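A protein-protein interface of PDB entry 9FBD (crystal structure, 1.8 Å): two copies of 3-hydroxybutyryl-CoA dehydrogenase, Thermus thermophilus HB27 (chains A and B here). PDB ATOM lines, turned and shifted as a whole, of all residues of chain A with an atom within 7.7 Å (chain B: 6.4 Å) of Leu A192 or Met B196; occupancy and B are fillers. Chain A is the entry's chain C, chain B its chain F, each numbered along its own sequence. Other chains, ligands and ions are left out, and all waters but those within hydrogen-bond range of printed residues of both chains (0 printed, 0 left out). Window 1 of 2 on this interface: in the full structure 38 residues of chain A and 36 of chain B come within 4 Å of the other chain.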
ATOM      1  N   PRO A 185       9.666  15.064  -0.919  1.00  0.00           N
ATOM      2  CA  PRO A 185       8.849  13.949  -0.441  1.00  0.00           C
ATOM      3  C   PRO A 185       7.509  13.839  -1.182  1.00  0.00           C
ATOM      4  O   PRO A 185       6.810  14.842  -1.357  1.00  0.00           O
ATOM      5  CB  PRO A 185       8.657  14.311   1.035  1.00  0.00           C
ATOM      6  CG  PRO A 185       9.894  15.129   1.374  1.00  0.00           C
ATOM      7  CD  PRO A 185      10.120  15.969   0.147  1.00  0.00           C
ATOM      8  N   GLY A 186       7.196  12.631  -1.644  1.00  0.00           N
ATOM      9  CA  GLY A 186       5.954  12.304  -2.377  1.00  0.00           C
ATOM     10  C   GLY A 186       5.988  12.738  -3.823  1.00  0.00           C
ATOM     11  O   GLY A 186       4.986  12.525  -4.523  1.00  0.00           O
ATOM     12  N   PHE A 187       7.076  13.359  -4.269  1.00  0.00           N
ATOM     13  CA  PHE A 187       7.215  13.885  -5.654  1.00  0.00           C
ATOM     14  C   PHE A 187       6.002  14.769  -5.943  1.00  0.00           C
ATOM     15  O   PHE A 187       5.720  15.667  -5.131  1.00  0.00           O
ATOM     16  CB  PHE A 187       7.420  12.705  -6.620  1.00  0.00           C
ATOM     17  CG  PHE A 187       8.448  11.693  -6.172  1.00  0.00           C
ATOM     18  CD1 PHE A 187       9.662  12.085  -5.632  1.00  0.00           C
ATOM     19  CD2 PHE A 187       8.189  10.334  -6.287  1.00  0.00           C
ATOM     20  CE1 PHE A 187      10.583  11.148  -5.206  1.00  0.00           C
ATOM     21  CE2 PHE A 187       9.113   9.403  -5.852  1.00  0.00           C
ATOM     22  CZ  PHE A 187      10.305   9.807  -5.313  1.00  0.00           C
ATOM     23  N   ILE A 188       5.256  14.519  -7.027  1.00  0.00           N
ATOM     24  CA  ILE A 188       3.898  15.087  -7.191  1.00  0.00           C
ATOM     25  C   ILE A 188       2.854  14.006  -6.930  1.00  0.00           C
ATOM     26  O   ILE A 188       1.927  14.262  -6.128  1.00  0.00           O
ATOM     27  CB  ILE A 188       3.715  15.755  -8.573  1.00  0.00           C
ATOM     28  CG1 ILE A 188       4.568  17.016  -8.722  1.00  0.00           C
ATOM     29  CG2 ILE A 188       2.246  16.023  -8.823  1.00  0.00           C
ATOM     30  CD1 ILE A 188       4.267  18.111  -7.696  1.00  0.00           C
ATOM     31  N   SER A 189       2.965  12.853  -7.591  1.00  0.00           N
ATOM     32  CA  SER A 189       1.899  11.811  -7.614  1.00  0.00           C
ATOM     33  C   SER A 189       1.426  11.480  -6.190  1.00  0.00           C
ATOM     34  O   SER A 189       0.234  11.631  -5.900  1.00  0.00           O
ATOM     35  CB  SER A 189       2.376  10.565  -8.327  1.00  0.00           C
ATOM     36  OG  SER A 189       3.615  10.104  -7.775  1.00  0.00           O
ATOM     37  N   ASN A 190       2.327  11.037  -5.329  1.00  0.00           N
ATOM     38  CA  ASN A 190       1.972  10.535  -3.967  1.00  0.00           C
ATOM     39  C   ASN A 190       1.717  11.700  -3.002  1.00  0.00           C
ATOM     40  O   ASN A 190       0.859  11.561  -2.133  1.00  0.00           O
ATOM     41  CB  ASN A 190       3.026   9.539  -3.480  1.00  0.00           C
ATOM     42  CG  ASN A 190       2.780   8.210  -4.197  1.00  0.00           C
ATOM     43  OD1 ASN A 190       1.629   7.802  -4.370  1.00  0.00           O
ATOM     44  ND2 ASN A 190       3.813   7.565  -4.681  1.00  0.00           N
ATOM     45  N   ARG A 191       2.400  12.819  -3.185  1.00  0.00           N
ATOM     46  CA  ARG A 191       2.189  14.027  -2.364  1.00  0.00           C
ATOM     47  C   ARG A 191       0.749  14.502  -2.524  1.00  0.00           C
ATOM     48  O   ARG A 191       0.189  14.992  -1.537  1.00  0.00           O
ATOM     49  CB  ARG A 191       3.177  15.111  -2.769  1.00  0.00           C
ATOM     50  CG  ARG A 191       2.914  16.416  -2.034  1.00  0.00           C
ATOM     51  CD  ARG A 191       3.954  17.428  -2.373  1.00  0.00           C
ATOM     52  NE  ARG A 191       3.679  18.667  -1.677  1.00  0.00           N
ATOM     53  CZ  ARG A 191       4.516  19.683  -1.645  1.00  0.00           C
ATOM     54  NH1 ARG A 191       5.688  19.591  -2.246  1.00  0.00           N
ATOM     55  NH2 ARG A 191       4.197  20.787  -0.987  1.00  0.00           N
ATOM     56  N   LEU A 192       0.158  14.368  -3.718  1.00  0.00           N
ATOM     57  CA  LEU A 192      -1.211  14.860  -3.982  1.00  0.00           C
ATOM     58  C   LEU A 192      -2.226  13.765  -3.616  1.00  0.00           C
ATOM     59  O   LEU A 192      -3.230  14.070  -2.913  1.00  0.00           O
ATOM     60  CB  LEU A 192      -1.313  15.328  -5.438  1.00  0.00           C
ATOM     61  CG  LEU A 192      -1.073  16.832  -5.671  1.00  0.00           C
ATOM     62  CD1 LEU A 192       0.076  17.386  -4.848  1.00  0.00           C
ATOM     63  CD2 LEU A 192      -0.845  17.154  -7.132  1.00  0.00           C
ATOM     64  N   LEU A 193      -1.958  12.523  -4.000  1.00  0.00           N
ATOM     65  CA  LEU A 193      -2.933  11.418  -3.815  1.00  0.00           C
ATOM     66  C   LEU A 193      -3.057  11.021  -2.339  1.00  0.00           C
ATOM     67  O   LEU A 193      -4.177  10.873  -1.853  1.00  0.00           O
ATOM     68  CB  LEU A 193      -2.494  10.195  -4.616  1.00  0.00           C
ATOM     69  CG  LEU A 193      -3.429   8.999  -4.445  1.00  0.00           C
ATOM     70  CD1 LEU A 193      -4.834   9.357  -4.923  1.00  0.00           C
ATOM     71  CD2 LEU A 193      -2.882   7.793  -5.167  1.00  0.00           C
ATOM     72  N   MET A 194      -1.945  10.772  -1.659  1.00  0.00           N
ATOM     73  CA  MET A 194      -2.015   9.993  -0.408  1.00  0.00           C
ATOM     74  C   MET A 194      -2.645  10.819   0.709  1.00  0.00           C
ATOM     75  O   MET A 194      -3.436  10.275   1.473  1.00  0.00           O
ATOM     76  CB  MET A 194      -0.661   9.419   0.007  1.00  0.00           C
ATOM     77  CG  MET A 194      -0.822   8.244   0.993  1.00  0.00           C
ATOM     78  SD  MET A 194      -1.876   6.896   0.362  1.00  0.00           S
ATOM     79  CE  MET A 194      -0.847   6.422  -1.031  1.00  0.00           C
ATOM     80  N   PRO A 195      -2.379  12.140   0.853  1.00  0.00           N
ATOM     81  CA  PRO A 195      -3.046  12.933   1.905  1.00  0.00           C
ATOM     82  C   PRO A 195      -4.573  12.986   1.782  1.00  0.00           C
ATOM     83  O   PRO A 195      -5.244  13.010   2.786  1.00  0.00           O
ATOM     84  CB  PRO A 195      -2.396  14.324   1.777  1.00  0.00           C
ATOM     85  CG  PRO A 195      -1.011  13.971   1.246  1.00  0.00           C
ATOM     86  CD  PRO A 195      -1.308  12.908   0.193  1.00  0.00           C
ATOM     87  N   MET A 196      -5.103  12.910   0.558  1.00  0.00           N
ATOM     88  CA  MET A 196      -6.563  12.850   0.345  1.00  0.00           C
ATOM     89  C   MET A 196      -7.106  11.482   0.820  1.00  0.00           C
ATOM     90  O   MET A 196      -8.152  11.453   1.496  1.00  0.00           O
ATOM     91  CB  MET A 196      -6.860  13.130  -1.129  1.00  0.00           C
ATOM     92  CG  MET A 196      -8.320  13.247  -1.441  1.00  0.00           C
ATOM     93  SD  MET A 196      -8.901  11.701  -2.099  1.00  0.00           S
ATOM     94  CE  MET A 196      -8.322  11.945  -3.780  1.00  0.00           C
ATOM     95  N   ILE A 197      -6.410  10.384   0.527  1.00  0.00           N
ATOM     96  CA  ILE A 197      -6.790   9.037   1.047  1.00  0.00           C
ATOM     97  C   ILE A 197      -6.744   9.088   2.575  1.00  0.00           C
ATOM     98  O   ILE A 197      -7.676   8.645   3.230  1.00  0.00           O
ATOM     99  CB  ILE A 197      -5.888   7.941   0.456  1.00  0.00           C
ATOM    100  CG1 ILE A 197      -6.198   7.767  -1.037  1.00  0.00           C
ATOM    101  CG2 ILE A 197      -6.023   6.650   1.242  1.00  0.00           C
ATOM    102  CD1 ILE A 197      -5.258   6.848  -1.778  1.00  0.00           C
ATOM    103  N   MET A 218     -16.944  10.624  -3.686  1.00  0.00           N
ATOM    104  CA  MET A 218     -15.767  10.949  -4.524  1.00  0.00           C
ATOM    105  C   MET A 218     -15.963  10.380  -5.943  1.00  0.00           C
ATOM    106  O   MET A 218     -15.546  11.052  -6.919  1.00  0.00           O
ATOM    107  CB  MET A 218     -14.473  10.440  -3.886  1.00  0.00           C
ATOM    108  CG  MET A 218     -14.210  11.068  -2.519  1.00  0.00           C
ATOM    109  SD  MET A 218     -14.344  12.882  -2.532  1.00  0.00           S
ATOM    110  CE  MET A 218     -12.892  13.270  -3.506  1.00  0.00           C
ATOM    111  N   MET A 222     -16.936  13.772  -7.824  1.00  0.00           N
ATOM    112  CA  MET A 222     -15.632  14.261  -8.327  1.00  0.00           C
ATOM    113  C   MET A 222     -15.217  13.442  -9.546  1.00  0.00           C
ATOM    114  O   MET A 222     -14.158  13.763 -10.118  1.00  0.00           O
ATOM    115  CB  MET A 222     -14.574  14.177  -7.215  1.00  0.00           C
ATOM    116  CG  MET A 222     -14.371  15.469  -6.429  1.00  0.00           C
ATOM    117  SD  MET A 222     -15.852  16.378  -5.893  1.00  0.00           S
ATOM    118  CE  MET A 222     -16.443  15.385  -4.517  1.00  0.00           C
ATOM    119  N   HIS A 224     -13.897  10.546  -9.677  1.00  0.00           N
ATOM    120  CA  HIS A 224     -12.741   9.646  -9.437  1.00  0.00           C
ATOM    121  C   HIS A 224     -13.218   8.239  -9.783  1.00  0.00           C
ATOM    122  O   HIS A 224     -14.323   7.872  -9.386  1.00  0.00           O
ATOM    123  CB  HIS A 224     -12.230   9.740  -7.991  1.00  0.00           C
ATOM    124  CG  HIS A 224     -11.641  11.057  -7.618  1.00  0.00           C
ATOM    125  ND1 HIS A 224     -11.460  12.090  -8.527  1.00  0.00           N
ATOM    126  CD2 HIS A 224     -11.155  11.497  -6.438  1.00  0.00           C
ATOM    127  CE1 HIS A 224     -10.918  13.120  -7.909  1.00  0.00           C
ATOM    128  NE2 HIS A 224     -10.727  12.785  -6.615  1.00  0.00           N
ATOM    129  N   LEU A 247       6.033  11.413   3.960  1.00  0.00           N
ATOM    130  CA  LEU A 247       5.593  12.834   3.901  1.00  0.00           C
ATOM    131  C   LEU A 247       5.798  13.461   5.277  1.00  0.00           C
ATOM    132  O   LEU A 247       6.356  14.573   5.356  1.00  0.00           O
ATOM    133  CB  LEU A 247       4.131  12.931   3.442  1.00  0.00           C
ATOM    134  CG  LEU A 247       3.863  12.388   2.033  1.00  0.00           C
ATOM    135  CD1 LEU A 247       2.396  12.465   1.686  1.00  0.00           C
ATOM    136  CD2 LEU A 247       4.665  13.145   0.997  1.00  0.00           C
ATOM    137  N   TYR A 256       1.016  16.237   7.686  1.00  0.00           N
ATOM    138  CA  TYR A 256       1.073  14.957   6.942  1.00  0.00           C
ATOM    139  C   TYR A 256       1.030  13.754   7.896  1.00  0.00           C
ATOM    140  O   TYR A 256       1.373  12.639   7.469  1.00  0.00           O
ATOM    141  CB  TYR A 256       2.316  14.901   6.050  1.00  0.00           C
ATOM    142  CG  TYR A 256       2.426  16.041   5.081  1.00  0.00           C
ATOM    143  CD1 TYR A 256       1.683  16.071   3.907  1.00  0.00           C
ATOM    144  CD2 TYR A 256       3.233  17.125   5.360  1.00  0.00           C
ATOM    145  CE1 TYR A 256       1.782  17.133   3.019  1.00  0.00           C
ATOM    146  CE2 TYR A 256       3.327  18.201   4.490  1.00  0.00           C
ATOM    147  CZ  TYR A 256       2.587  18.210   3.319  1.00  0.00           C
ATOM    148  OH  TYR A 256       2.677  19.276   2.460  1.00  0.00           O
ATOM    149  N   ARG B 191     -13.837  18.686   2.042  1.00  0.00           N
ATOM    150  CA  ARG B 191     -12.783  18.268   2.992  1.00  0.00           C
ATOM    151  C   ARG B 191     -11.758  17.375   2.282  1.00  0.00           C
ATOM    152  O   ARG B 191     -10.566  17.453   2.631  1.00  0.00           O
ATOM    153  CB  ARG B 191     -13.421  17.550   4.173  1.00  0.00           C
ATOM    154  CG  ARG B 191     -12.397  16.915   5.094  1.00  0.00           C
ATOM    155  CD  ARG B 191     -13.023  16.434   6.344  1.00  0.00           C
ATOM    156  NE  ARG B 191     -12.022  15.902   7.228  1.00  0.00           N
ATOM    157  CZ  ARG B 191     -12.281  15.450   8.442  1.00  0.00           C
ATOM    158  NH1 ARG B 191     -13.518  15.481   8.912  1.00  0.00           N
ATOM    159  NH2 ARG B 191     -11.299  14.967   9.178  1.00  0.00           N
ATOM    160  N   LEU B 192     -12.186  16.557   1.319  1.00  0.00           N
ATOM    161  CA  LEU B 192     -11.276  15.616   0.617  1.00  0.00           C
ATOM    162  C   LEU B 192     -10.650  16.328  -0.593  1.00  0.00           C
ATOM    163  O   LEU B 192      -9.400  16.267  -0.766  1.00  0.00           O
ATOM    164  CB  LEU B 192     -12.059  14.353   0.240  1.00  0.00           C
ATOM    165  CG  LEU B 192     -11.956  13.177   1.205  1.00  0.00           C
ATOM    166  CD1 LEU B 192     -12.010  13.623   2.658  1.00  0.00           C
ATOM    167  CD2 LEU B 192     -13.022  12.122   0.891  1.00  0.00           C
ATOM    168  N   LEU B 193     -11.462  17.046  -1.361  1.00  0.00           N
ATOM    169  CA  LEU B 193     -11.003  17.649  -2.634  1.00  0.00           C
ATOM    170  C   LEU B 193     -10.072  18.837  -2.374  1.00  0.00           C
ATOM    171  O   LEU B 193      -9.040  18.926  -3.020  1.00  0.00           O
ATOM    172  CB  LEU B 193     -12.200  18.120  -3.451  1.00  0.00           C
ATOM    173  CG  LEU B 193     -11.800  18.803  -4.755  1.00  0.00           C
ATOM    174  CD1 LEU B 193     -11.043  17.829  -5.653  1.00  0.00           C
ATOM    175  CD2 LEU B 193     -13.007  19.408  -5.452  1.00  0.00           C
ATOM    176  N   MET B 194     -10.466  19.783  -1.536  1.00  0.00           N
ATOM    177  CA  MET B 194      -9.832  21.122  -1.592  1.00  0.00           C
ATOM    178  C   MET B 194      -8.406  21.064  -1.031  1.00  0.00           C
ATOM    179  O   MET B 194      -7.519  21.703  -1.602  1.00  0.00           O
ATOM    180  CB  MET B 194     -10.665  22.202  -0.893  1.00  0.00           C
ATOM    181  CG  MET B 194     -10.256  23.610  -1.332  1.00  0.00           C
ATOM    182  SD  MET B 194     -10.383  23.856  -3.138  1.00  0.00           S
ATOM    183  CE  MET B 194     -12.136  23.568  -3.364  1.00  0.00           C
ATOM    184  N   PRO B 195      -8.093  20.309   0.044  1.00  0.00           N
ATOM    185  CA  PRO B 195      -6.699  20.200   0.502  1.00  0.00           C
ATOM    186  C   PRO B 195      -5.729  19.619  -0.536  1.00  0.00           C
ATOM    187  O   PRO B 195      -4.584  20.029  -0.582  1.00  0.00           O
ATOM    188  CB  PRO B 195      -6.807  19.323   1.764  1.00  0.00           C
ATOM    189  CG  PRO B 195      -8.203  19.607   2.259  1.00  0.00           C
ATOM    190  CD  PRO B 195      -9.034  19.651   0.980  1.00  0.00           C
ATOM    191  N   MET B 196      -6.195  18.735  -1.409  1.00  0.00           N
ATOM    192  CA  MET B 196      -5.364  18.201  -2.517  1.00  0.00           C
ATOM    193  C   MET B 196      -5.109  19.317  -3.557  1.00  0.00           C
ATOM    194  O   MET B 196      -3.978  19.457  -4.017  1.00  0.00           O
ATOM    195  CB  MET B 196      -6.042  16.968  -3.121  1.00  0.00           C
ATOM    196  CG  MET B 196      -5.168  16.258  -4.126  1.00  0.00           C
ATOM    197  SD  MET B 196      -5.632  16.763  -5.786  1.00  0.00           S
ATOM    198  CE  MET B 196      -7.050  15.676  -5.938  1.00  0.00           C
ATOM    199  N   ILE B 197      -6.121  20.114  -3.911  1.00  0.00           N
ATOM    200  CA  ILE B 197      -5.933  21.284  -4.811  1.00  0.00           C
ATOM    201  C   ILE B 197      -4.927  22.241  -4.159  1.00  0.00           C
ATOM    202  O   ILE B 197      -3.990  22.683  -4.813  1.00  0.00           O
ATOM    203  CB  ILE B 197      -7.270  21.958  -5.134  1.00  0.00           C
ATOM    204  CG1 ILE B 197      -8.110  21.044  -6.039  1.00  0.00           C
ATOM    205  CG2 ILE B 197      -7.047  23.333  -5.753  1.00  0.00           C
ATOM    206  CD1 ILE B 197      -9.527  21.525  -6.270  1.00  0.00           C
ATOM    207  N   ASN B 198      -5.131  22.538  -2.884  1.00  0.00           N
ATOM    208  CA  ASN B 198      -4.234  23.418  -2.099  1.00  0.00           C
ATOM    209  C   ASN B 198      -2.795  22.885  -2.125  1.00  0.00           C
ATOM    210  O   ASN B 198      -1.857  23.691  -2.266  1.00  0.00           O
ATOM    211  CB  ASN B 198      -4.772  23.569  -0.682  1.00  0.00           C
ATOM    212  CG  ASN B 198      -4.075  24.668   0.066  1.00  0.00           C
ATOM    213  OD1 ASN B 198      -4.202  25.829  -0.310  1.00  0.00           O
ATOM    214  ND2 ASN B 198      -3.317  24.297   1.079  1.00  0.00           N
ATOM    215  N   GLU B 199      -2.608  21.573  -1.994  1.00  0.00           N
ATOM    216  CA  GLU B 199      -1.280  20.930  -2.015  1.00  0.00           C
ATOM    217  C   GLU B 199      -0.647  21.076  -3.402  1.00  0.00           C
ATOM    218  O   GLU B 199       0.569  21.306  -3.483  1.00  0.00           O
ATOM    219  CB  GLU B 199      -1.405  19.442  -1.649  1.00  0.00           C
ATOM    220  CG  GLU B 199      -0.058  18.808  -1.333  1.00  0.00           C
ATOM    221  CD  GLU B 199       0.508  19.277   0.001  1.00  0.00           C
ATOM    222  OE1 GLU B 199      -0.277  19.687   0.857  1.00  0.00           O
ATOM    223  OE2 GLU B 199       1.707  19.196   0.177  1.00  0.00           O
ATOM    224  N   ALA B 200      -1.428  20.953  -4.471  1.00  0.00           N
ATOM    225  CA  ALA B 200      -0.914  21.170  -5.839  1.00  0.00           C
ATOM    226  C   ALA B 200      -0.385  22.610  -5.954  1.00  0.00           C
ATOM    227  O   ALA B 200       0.700  22.837  -6.534  1.00  0.00           O
ATOM    228  CB  ALA B 200      -2.020  20.895  -6.842  1.00  0.00           C
ATOM    229  N   ILE B 201      -1.118  23.562  -5.398  1.00  0.00           N
ATOM    230  CA  ILE B 201      -0.733  24.999  -5.468  1.00  0.00           C
ATOM    231  C   ILE B 201       0.566  25.187  -4.660  1.00  0.00           C
ATOM    232  O   ILE B 201       1.450  25.867  -5.155  1.00  0.00           O
ATOM    233  CB  ILE B 201      -1.887  25.905  -4.993  1.00  0.00           C
ATOM    234  CG1 ILE B 201      -3.105  25.770  -5.901  1.00  0.00           C
ATOM    235  CG2 ILE B 201      -1.435  27.349  -4.881  1.00  0.00           C
ATOM    236  CD1 ILE B 201      -4.378  26.378  -5.327  1.00  0.00           C
ATOM    237  N   ALA B 203       2.927  22.807  -4.063  1.00  0.00           N
ATOM    238  CA  ALA B 203       3.974  22.171  -4.895  1.00  0.00           C
ATOM    239  C   ALA B 203       4.394  23.128  -6.013  1.00  0.00           C
ATOM    240  O   ALA B 203       5.610  23.225  -6.291  1.00  0.00           O
ATOM    241  CB  ALA B 203       3.496  20.849  -5.442  1.00  0.00           C
ATOM    242  N   ILE B 214       2.102  19.051 -13.172  1.00  0.00           N
ATOM    243  CA  ILE B 214       1.220  18.716 -12.026  1.00  0.00           C
ATOM    244  C   ILE B 214      -0.120  18.224 -12.565  1.00  0.00           C
ATOM    245  O   ILE B 214      -0.565  17.154 -12.134  1.00  0.00           O
ATOM    246  CB  ILE B 214       1.074  19.914 -11.069  1.00  0.00           C
ATOM    247  CG1 ILE B 214       2.399  20.172 -10.347  1.00  0.00           C
ATOM    248  CG2 ILE B 214      -0.079  19.682 -10.113  1.00  0.00           C
ATOM    249  CD1 ILE B 214       2.454  21.525  -9.648  1.00  0.00           C
ATOM    250  N   ILE B 217       0.228  14.825 -14.474  1.00  0.00           N
ATOM    251  CA  ILE B 217       0.498  13.680 -13.566  1.00  0.00           C
ATOM    252  C   ILE B 217      -0.837  13.226 -12.964  1.00  0.00           C
ATOM    253  O   ILE B 217      -1.079  12.006 -12.937  1.00  0.00           O
ATOM    254  CB  ILE B 217       1.556  14.029 -12.518  1.00  0.00           C
ATOM    255  CG1 ILE B 217       2.937  14.067 -13.167  1.00  0.00           C
ATOM    256  CG2 ILE B 217       1.496  13.064 -11.340  1.00  0.00           C
ATOM    257  CD1 ILE B 217       3.988  14.780 -12.347  1.00  0.00           C
ATOM    258  N   MET B 218      -1.695  14.144 -12.538  1.00  0.00           N
ATOM    259  CA  MET B 218      -2.954  13.740 -11.869  1.00  0.00           C
ATOM    260  C   MET B 218      -3.948  13.197 -12.921  1.00  0.00           C
ATOM    261  O   MET B 218      -4.668  12.225 -12.611  1.00  0.00           O
ATOM    262  CB  MET B 218      -3.557  14.895 -11.061  1.00  0.00           C
ATOM    263  CG  MET B 218      -2.614  15.378  -9.964  1.00  0.00           C
ATOM    264  SD  MET B 218      -1.954  14.025  -8.917  1.00  0.00           S
ATOM    265  CE  MET B 218      -3.457  13.549  -8.069  1.00  0.00           C
ATOM    266  N   HIS B 224      -7.790  11.352 -12.926  1.00  0.00           N
ATOM    267  CA  HIS B 224      -8.680  12.501 -12.620  1.00  0.00           C
ATOM    268  C   HIS B 224      -9.033  13.144 -13.957  1.00  0.00           C
ATOM    269  O   HIS B 224      -8.154  13.300 -14.795  1.00  0.00           O
ATOM    270  CB  HIS B 224      -8.016  13.496 -11.661  1.00  0.00           C
ATOM    271  CG  HIS B 224      -7.760  12.976 -10.286  1.00  0.00           C
ATOM    272  ND1 HIS B 224      -8.181  11.726  -9.862  1.00  0.00           N
ATOM    273  CD2 HIS B 224      -7.124  13.537  -9.232  1.00  0.00           C
ATOM    274  CE1 HIS B 224      -7.809  11.541  -8.609  1.00  0.00           C
ATOM    275  NE2 HIS B 224      -7.159  12.636  -8.200  1.00  0.00           N
ATOM    276  N   PRO B 228      -5.608  19.277 -10.676  1.00  0.00           N
ATOM    277  CA  PRO B 228      -6.054  20.162  -9.596  1.00  0.00           C
ATOM    278  C   PRO B 228      -5.934  21.672  -9.897  1.00  0.00           C
ATOM    279  O   PRO B 228      -6.721  22.437  -9.374  1.00  0.00           O
ATOM    280  CB  PRO B 228      -5.148  19.759  -8.420  1.00  0.00           C
ATOM    281  CG  PRO B 228      -3.938  19.133  -9.067  1.00  0.00           C
ATOM    282  CD  PRO B 228      -4.457  18.445 -10.297  1.00  0.00           C
ATOM    283  N   MET B 244     -10.737  26.596   1.926  1.00  0.00           N
ATOM    284  CA  MET B 244      -9.543  26.299   2.749  1.00  0.00           C
ATOM    285  C   MET B 244      -9.637  27.100   4.057  1.00  0.00           C
ATOM    286  O   MET B 244      -9.339  26.531   5.117  1.00  0.00           O
ATOM    287  CB  MET B 244      -8.238  26.601   2.011  1.00  0.00           C
ATOM    288  CG  MET B 244      -7.872  25.614   0.897  1.00  0.00           C
ATOM    289  SD  MET B 244      -7.975  23.860   1.379  1.00  0.00           S
ATOM    290  CE  MET B 244      -6.742  23.760   2.679  1.00  0.00           C
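The guanidinium group (NE) of Arg A191 is in salt-bridge range of the side-chain carboxylate (OE2) of Glu B199, 2.8 Å away. The side-chain hydroxyl (OH) of Tyr A256 lies within hydrogen-bond range of the side-chain carboxylate (OE2) of Glu B199.
O of Gly A186 sits at hydrogen-bond distance from N of Arg A191, 2.9 Å away. The backbone carbonyl oxygen of Met A218 sits at hydrogen-bond distance from the backbone NH of His A224, at 3.3 Å. The backbone NH of His B224 is in hydrogen-bond range of the backbone carbonyl oxygen of Met B218 (3.3 Å).
Ile A188 touches Ala B203. Ile B217 touches Ile A188 (CD1 to CB, 3.9 Å). Ala B203 touches Arg A191. Leu A192 touches Met B196 (O to CG, 3.2 Å). Glu B199 touches Leu A192 (CG to CD1, 3.8 Å). CD1 of Leu A192 touches N of Ala B200 (3.9 Å). Leu A192 touches Ile B214 (CD2 to CG2, 3.98 Å). CD2 of Leu A192 touches SD of Met B218, at 3.8 Å. SD of Met A218 touches CD2 of Leu B192, at 3.7 Å. His A224 touches His B224 (CE1 to CE1, 3.6 Å).
Asn A190 touches none of the printed residues of chain B. Of the printed residues of chain B, Leu A192 touches Met B196, Glu B199, Ala B200, Ile B214 and Met B218. Of the printed residues of chain B, His A224 touches His B224. Of the printed residues of chain B, Tyr A256 touches Glu B199. Of the printed residues of chain A, Met B196 touches Leu A192. The nearest printed residue of chain B that does not touch Leu A192 is Pro B228 (4.2 Å). The nearest residue of chain A that does not touch Met B196 is Met A196 (4.4 Å). The nearest printed residue of chain A that does not touch Ala B203 is Leu A192 (4.9 Å).
Printed residues of chain A that touch a printed residue of chain B: Ile A188, Ser A189, Arg A191, Leu A192, Met A196, Met A218, His A224 and Tyr A256. Printed residues of chain B that touch a printed residue of chain A: Leu B192, Met B196, Glu B199, Ala B200, Ala B203, Ile B214, Ile B217, Met B218 and His B224.
Leu A192 touches Met B196, and with the chains exchanged Met A196 touches Leu B192. Leu A192 touches Met B218, and with the chains exchanged Met A218 touches Leu B192. His A224 touches its own counterpart, His B224. Positions printed for both chains: 191, 192, 193, 194, 195, 196, 197, 218 and 224. Of the 15 pairs that touch across the chains among the printed residues, 5 have their exchanged pair printed and touching as well.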
